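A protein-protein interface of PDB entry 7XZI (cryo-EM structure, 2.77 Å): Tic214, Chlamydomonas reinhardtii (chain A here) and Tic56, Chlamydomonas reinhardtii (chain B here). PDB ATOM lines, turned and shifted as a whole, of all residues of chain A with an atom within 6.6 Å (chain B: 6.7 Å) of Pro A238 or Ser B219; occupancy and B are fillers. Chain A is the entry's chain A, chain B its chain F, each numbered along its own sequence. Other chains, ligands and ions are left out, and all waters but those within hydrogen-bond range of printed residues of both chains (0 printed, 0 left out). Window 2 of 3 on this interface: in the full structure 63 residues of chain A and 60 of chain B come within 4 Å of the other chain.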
ATOM      1  N   ILE A 114     -11.364  31.799  -2.860  1.00  0.00           N
ATOM      2  CA  ILE A 114     -11.098  30.957  -4.022  1.00  0.00           C
ATOM      3  C   ILE A 114     -11.129  31.783  -5.301  1.00  0.00           C
ATOM      4  O   ILE A 114     -10.300  31.595  -6.196  1.00  0.00           O
ATOM      5  CB  ILE A 114     -12.093  29.781  -4.071  1.00  0.00           C
ATOM      6  CG1 ILE A 114     -11.774  28.774  -2.963  1.00  0.00           C
ATOM      7  CG2 ILE A 114     -12.056  29.097  -5.425  1.00  0.00           C
ATOM      8  CD1 ILE A 114     -12.713  27.585  -2.922  1.00  0.00           C
ATOM      9  N   SER A 235      -6.982  25.801 -11.962  1.00  0.00           N
ATOM     10  CA  SER A 235      -7.846  26.418 -10.969  1.00  0.00           C
ATOM     11  C   SER A 235      -7.618  25.733  -9.632  1.00  0.00           C
ATOM     12  O   SER A 235      -7.453  24.511  -9.575  1.00  0.00           O
ATOM     13  CB  SER A 235      -9.322  26.323 -11.371  1.00  0.00           C
ATOM     14  OG  SER A 235      -9.726  24.972 -11.501  1.00  0.00           O
ATOM     15  N   PHE A 236      -7.610  26.524  -8.559  1.00  0.00           N
ATOM     16  CA  PHE A 236      -7.417  25.996  -7.209  1.00  0.00           C
ATOM     17  C   PHE A 236      -8.747  25.505  -6.632  1.00  0.00           C
ATOM     18  O   PHE A 236      -9.281  26.032  -5.657  1.00  0.00           O
ATOM     19  CB  PHE A 236      -6.777  27.052  -6.317  1.00  0.00           C
ATOM     20  CG  PHE A 236      -5.291  27.182  -6.502  1.00  0.00           C
ATOM     21  CD1 PHE A 236      -4.771  27.891  -7.571  1.00  0.00           C
ATOM     22  CD2 PHE A 236      -4.415  26.598  -5.602  1.00  0.00           C
ATOM     23  CE1 PHE A 236      -3.405  28.012  -7.742  1.00  0.00           C
ATOM     24  CE2 PHE A 236      -3.048  26.716  -5.768  1.00  0.00           C
ATOM     25  CZ  PHE A 236      -2.542  27.424  -6.839  1.00  0.00           C
ATOM     26  N   GLY A 237      -9.279  24.462  -7.264  1.00  0.00           N
ATOM     27  CA  GLY A 237     -10.519  23.860  -6.839  1.00  0.00           C
ATOM     28  C   GLY A 237     -10.771  22.548  -7.552  1.00  0.00           C
ATOM     29  O   GLY A 237     -10.100  22.206  -8.530  1.00  0.00           O
ATOM     30  N   PRO A 238     -11.750  21.781  -7.073  1.00  0.00           N
ATOM     31  CA  PRO A 238     -12.065  20.478  -7.690  1.00  0.00           C
ATOM     32  C   PRO A 238     -12.880  20.621  -8.971  1.00  0.00           C
ATOM     33  O   PRO A 238     -13.972  20.063  -9.115  1.00  0.00           O
ATOM     34  CB  PRO A 238     -12.844  19.764  -6.574  1.00  0.00           C
ATOM     35  CG  PRO A 238     -12.656  20.594  -5.329  1.00  0.00           C
ATOM     36  CD  PRO A 238     -12.482  21.985  -5.815  1.00  0.00           C
ATOM     37  N   ASP A 239     -12.342  21.378  -9.925  1.00  0.00           N
ATOM     38  CA  ASP A 239     -13.004  21.630 -11.196  1.00  0.00           C
ATOM     39  C   ASP A 239     -11.984  21.497 -12.319  1.00  0.00           C
ATOM     40  O   ASP A 239     -10.796  21.256 -12.085  1.00  0.00           O
ATOM     41  CB  ASP A 239     -13.663  23.017 -11.215  1.00  0.00           C
ATOM     42  CG  ASP A 239     -14.780  23.151 -10.197  1.00  0.00           C
ATOM     43  OD1 ASP A 239     -15.562  22.190 -10.036  1.00  0.00           O
ATOM     44  OD2 ASP A 239     -14.879  24.218  -9.557  1.00  0.00           O
ATOM     45  N   ALA A 240     -12.460  21.657 -13.554  1.00  0.00           N
ATOM     46  CA  ALA A 240     -11.600  21.612 -14.728  1.00  0.00           C
ATOM     47  C   ALA A 240     -11.167  22.990 -15.207  1.00  0.00           C
ATOM     48  O   ALA A 240     -10.170  23.094 -15.929  1.00  0.00           O
ATOM     49  CB  ALA A 240     -12.303  20.882 -15.877  1.00  0.00           C
ATOM     50  N   GLU A 244     -16.685  26.976 -14.019  1.00  0.00           N
ATOM     51  CA  GLU A 244     -17.691  26.076 -13.475  1.00  0.00           C
ATOM     52  C   GLU A 244     -18.190  26.579 -12.126  1.00  0.00           C
ATOM     53  O   GLU A 244     -17.420  27.107 -11.319  1.00  0.00           O
ATOM     54  CB  GLU A 244     -17.127  24.664 -13.336  1.00  0.00           C
ATOM     55  CG  GLU A 244     -16.637  24.069 -14.645  1.00  0.00           C
ATOM     56  CD  GLU A 244     -16.226  22.619 -14.507  1.00  0.00           C
ATOM     57  OE1 GLU A 244     -16.552  22.006 -13.469  1.00  0.00           O
ATOM     58  OE2 GLU A 244     -15.577  22.092 -15.436  1.00  0.00           O
ATOM     59  N   LYS B 211      -1.503  20.612  -9.982  1.00  0.00           N
ATOM     60  CA  LYS B 211      -2.913  20.324  -9.739  1.00  0.00           C
ATOM     61  C   LYS B 211      -3.082  19.265  -8.656  1.00  0.00           C
ATOM     62  O   LYS B 211      -3.969  19.369  -7.802  1.00  0.00           O
ATOM     63  CB  LYS B 211      -3.581  19.876 -11.040  1.00  0.00           C
ATOM     64  CG  LYS B 211      -5.079  19.641 -10.937  1.00  0.00           C
ATOM     65  CD  LYS B 211      -5.841  20.948 -10.807  1.00  0.00           C
ATOM     66  CE  LYS B 211      -7.341  20.709 -10.801  1.00  0.00           C
ATOM     67  NZ  LYS B 211      -8.105  21.985 -10.768  1.00  0.00           N
ATOM     68  N   PHE B 214      -1.664  20.938  -5.009  1.00  0.00           N
ATOM     69  CA  PHE B 214      -2.265  22.115  -4.402  1.00  0.00           C
ATOM     70  C   PHE B 214      -3.777  22.209  -4.537  1.00  0.00           C
ATOM     71  O   PHE B 214      -4.382  23.055  -3.869  1.00  0.00           O
ATOM     72  CB  PHE B 214      -1.640  23.392  -4.987  1.00  0.00           C
ATOM     73  CG  PHE B 214      -0.191  23.562  -4.644  1.00  0.00           C
ATOM     74  CD1 PHE B 214       0.186  24.160  -3.454  1.00  0.00           C
ATOM     75  CD2 PHE B 214       0.796  23.120  -5.509  1.00  0.00           C
ATOM     76  CE1 PHE B 214       1.519  24.315  -3.133  1.00  0.00           C
ATOM     77  CE2 PHE B 214       2.130  23.274  -5.194  1.00  0.00           C
ATOM     78  CZ  PHE B 214       2.492  23.872  -4.005  1.00  0.00           C
ATOM     79  N   SER B 215      -4.410  21.385  -5.371  1.00  0.00           N
ATOM     80  CA  SER B 215      -5.856  21.488  -5.529  1.00  0.00           C
ATOM     81  C   SER B 215      -6.584  20.223  -5.092  1.00  0.00           C
ATOM     82  O   SER B 215      -7.492  20.281  -4.258  1.00  0.00           O
ATOM     83  CB  SER B 215      -6.207  21.815  -6.982  1.00  0.00           C
ATOM     84  OG  SER B 215      -7.606  21.962  -7.146  1.00  0.00           O
ATOM     85  N   LEU B 216      -6.198  19.075  -5.651  1.00  0.00           N
ATOM     86  CA  LEU B 216      -6.953  17.851  -5.403  1.00  0.00           C
ATOM     87  C   LEU B 216      -6.648  17.261  -4.031  1.00  0.00           C
ATOM     88  O   LEU B 216      -7.553  16.762  -3.356  1.00  0.00           O
ATOM     89  CB  LEU B 216      -6.675  16.830  -6.505  1.00  0.00           C
ATOM     90  CG  LEU B 216      -7.226  17.215  -7.879  1.00  0.00           C
ATOM     91  CD1 LEU B 216      -7.039  16.088  -8.878  1.00  0.00           C
ATOM     92  CD2 LEU B 216      -8.692  17.607  -7.777  1.00  0.00           C
ATOM     93  N   LYS B 217      -5.378  17.286  -3.611  1.00  0.00           N
ATOM     94  CA  LYS B 217      -5.023  16.676  -2.329  1.00  0.00           C
ATOM     95  C   LYS B 217      -5.668  17.384  -1.141  1.00  0.00           C
ATOM     96  O   LYS B 217      -6.236  16.693  -0.273  1.00  0.00           O
ATOM     97  CB  LYS B 217      -3.499  16.602  -2.195  1.00  0.00           C
ATOM     98  CG  LYS B 217      -3.009  15.460  -1.321  1.00  0.00           C
ATOM     99  CD  LYS B 217      -1.492  15.365  -1.329  1.00  0.00           C
ATOM    100  CE  LYS B 217      -1.013  14.103  -0.629  1.00  0.00           C
ATOM    101  NZ  LYS B 217      -1.457  12.874  -1.343  1.00  0.00           N
ATOM    102  N   PRO B 218      -5.602  18.717  -1.008  1.00  0.00           N
ATOM    103  CA  PRO B 218      -6.313  19.356   0.113  1.00  0.00           C
ATOM    104  C   PRO B 218      -7.815  19.144   0.065  1.00  0.00           C
ATOM    105  O   PRO B 218      -8.448  19.001   1.118  1.00  0.00           O
ATOM    106  CB  PRO B 218      -5.937  20.837  -0.031  1.00  0.00           C
ATOM    107  CG  PRO B 218      -5.582  20.997  -1.459  1.00  0.00           C
ATOM    108  CD  PRO B 218      -4.903  19.718  -1.836  1.00  0.00           C
ATOM    109  N   SER B 219      -8.405  19.116  -1.131  1.00  0.00           N
ATOM    110  CA  SER B 219      -9.840  18.866  -1.239  1.00  0.00           C
ATOM    111  C   SER B 219     -10.187  17.451  -0.794  1.00  0.00           C
ATOM    112  O   SER B 219     -11.215  17.234  -0.143  1.00  0.00           O
ATOM    113  CB  SER B 219     -10.309  19.114  -2.672  1.00  0.00           C
ATOM    114  OG  SER B 219     -10.103  20.464  -3.048  1.00  0.00           O
ATOM    115  N   LEU B 220      -9.342  16.477  -1.137  1.00  0.00           N
ATOM    116  CA  LEU B 220      -9.554  15.111  -0.674  1.00  0.00           C
ATOM    117  C   LEU B 220      -9.437  15.024   0.841  1.00  0.00           C
ATOM    118  O   LEU B 220     -10.239  14.347   1.496  1.00  0.00           O
ATOM    119  CB  LEU B 220      -8.558  14.166  -1.347  1.00  0.00           C
ATOM    120  CG  LEU B 220      -8.681  12.683  -0.993  1.00  0.00           C
ATOM    121  CD1 LEU B 220     -10.062  12.163  -1.359  1.00  0.00           C
ATOM    122  CD2 LEU B 220      -7.597  11.868  -1.684  1.00  0.00           C
ATOM    123  N   ASN B 221      -8.448  15.707   1.419  1.00  0.00           N
ATOM    124  CA  ASN B 221      -8.324  15.723   2.876  1.00  0.00           C
ATOM    125  C   ASN B 221      -9.557  16.347   3.522  1.00  0.00           C
ATOM    126  O   ASN B 221     -10.081  15.832   4.518  1.00  0.00           O
ATOM    127  CB  ASN B 221      -7.059  16.474   3.290  1.00  0.00           C
ATOM    128  CG  ASN B 221      -5.792  15.774   2.843  1.00  0.00           C
ATOM    129  OD1 ASN B 221      -5.779  14.561   2.634  1.00  0.00           O
ATOM    130  ND2 ASN B 221      -4.715  16.537   2.696  1.00  0.00           N
ATOM    131  N   ARG B 222     -10.040  17.457   2.956  1.00  0.00           N
ATOM    132  CA  ARG B 222     -11.208  18.134   3.509  1.00  0.00           C
ATOM    133  C   ARG B 222     -12.455  17.264   3.413  1.00  0.00           C
ATOM    134  O   ARG B 222     -13.255  17.211   4.354  1.00  0.00           O
ATOM    135  CB  ARG B 222     -11.425  19.467   2.794  1.00  0.00           C
ATOM    136  CG  ARG B 222     -12.625  20.257   3.292  1.00  0.00           C
ATOM    137  CD  ARG B 222     -12.751  21.602   2.587  1.00  0.00           C
ATOM    138  NE  ARG B 222     -11.649  22.501   2.901  1.00  0.00           N
ATOM    139  CZ  ARG B 222     -10.598  22.708   2.114  1.00  0.00           C
ATOM    140  NH1 ARG B 222     -10.479  22.096   0.947  1.00  0.00           N
ATOM    141  NH2 ARG B 222      -9.648  23.548   2.508  1.00  0.00           N
ATOM    142  N   ILE B 223     -12.646  16.579   2.283  1.00  0.00           N
ATOM    143  CA  ILE B 223     -13.836  15.747   2.131  1.00  0.00           C
ATOM    144  C   ILE B 223     -13.746  14.509   3.018  1.00  0.00           C
ATOM    145  O   ILE B 223     -14.771  14.014   3.503  1.00  0.00           O
ATOM    146  CB  ILE B 223     -14.068  15.387   0.649  1.00  0.00           C
ATOM    147  CG1 ILE B 223     -15.481  14.835   0.450  1.00  0.00           C
ATOM    148  CG2 ILE B 223     -13.042  14.389   0.147  1.00  0.00           C
ATOM    149  CD1 ILE B 223     -16.570  15.833   0.762  1.00  0.00           C
ATOM    150  N   ARG B 224     -12.537  13.985   3.247  1.00  0.00           N
ATOM    151  CA  ARG B 224     -12.384  12.884   4.193  1.00  0.00           C
ATOM    152  C   ARG B 224     -12.700  13.331   5.615  1.00  0.00           C
ATOM    153  O   ARG B 224     -13.342  12.597   6.374  1.00  0.00           O
ATOM    154  CB  ARG B 224     -10.969  12.313   4.113  1.00  0.00           C
ATOM    155  CG  ARG B 224     -10.710  11.476   2.875  1.00  0.00           C
ATOM    156  CD  ARG B 224      -9.260  11.038   2.800  1.00  0.00           C
ATOM    157  NE  ARG B 224      -9.021  10.154   1.669  1.00  0.00           N
ATOM    158  CZ  ARG B 224      -7.825   9.693   1.317  1.00  0.00           C
ATOM    159  NH1 ARG B 224      -6.733  10.024   1.985  1.00  0.00           N
ATOM    160  NH2 ARG B 224      -7.727   8.882   0.270  1.00  0.00           N
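NZ of Lys B211 is in hydrogen-bond range of O of Ser A235 (2.9 Å). The side-chain amino group of Lys B211 is in hydrogen-bond range of the backbone carbonyl oxygen of Gly A237. The backbone carbonyl oxygen (O) of Asp A239 lies within hydrogen-bond range of the side-chain amino group (NZ) of Lys B211. The side-chain hydroxyl of Ser B215 lies within hydrogen-bond range of the backbone carbonyl oxygen of Gly A237.
N of Leu B216 is in hydrogen-bond range of O of Lys B211, at 3.1 Å. The side-chain hydroxyl (OG) of Ser B219 sits at hydrogen-bond distance from the backbone carbonyl oxygen (O) of Ser B215 (2.9 Å).
O of Ser A235 touches OG of Ser B215, at 3.5 Å. CB of Phe B214 touches CE2 of Phe A236, at 3.7 Å. Phe A236 touches Ser B215 (C to OG, 3.8 Å). Pro A238 touches Ser B219.
Pro A238 touches just one residue of chain B: Ser B219. Printed residues of chain B within 4 Å of Asp A239: Lys B211 (3.1 Å). Of the printed residues of chain A, Lys B211 touches Ser A235, Gly A237 and Asp A239. Of the printed residues of chain A, Phe B214 touches Phe A236 (3.7 Å). Ser B219 touches just one residue of chain A: Pro A238. The nearest residue of chain B that does not touch Pro A238 is Ser B215 (4.1 Å). The nearest residue of chain A that does not touch Ser B219 is Gly A237 (5.0 Å). The nearest printed residue of chain A that does not touch Ser B215 is Pro A238 (4.1 Å).
Of the 8 printed residues of chain A, 5 touch a printed residue of chain B. Along chain A the printed residues that touch a printed residue of chain B span positions 235 to 239. Of the 12 printed residues of chain B, 4 touch a printed residue of chain A. Hydrophobic or aromatic side chains of chain B within 4 Å of the printed part of chain A: Phe B214.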
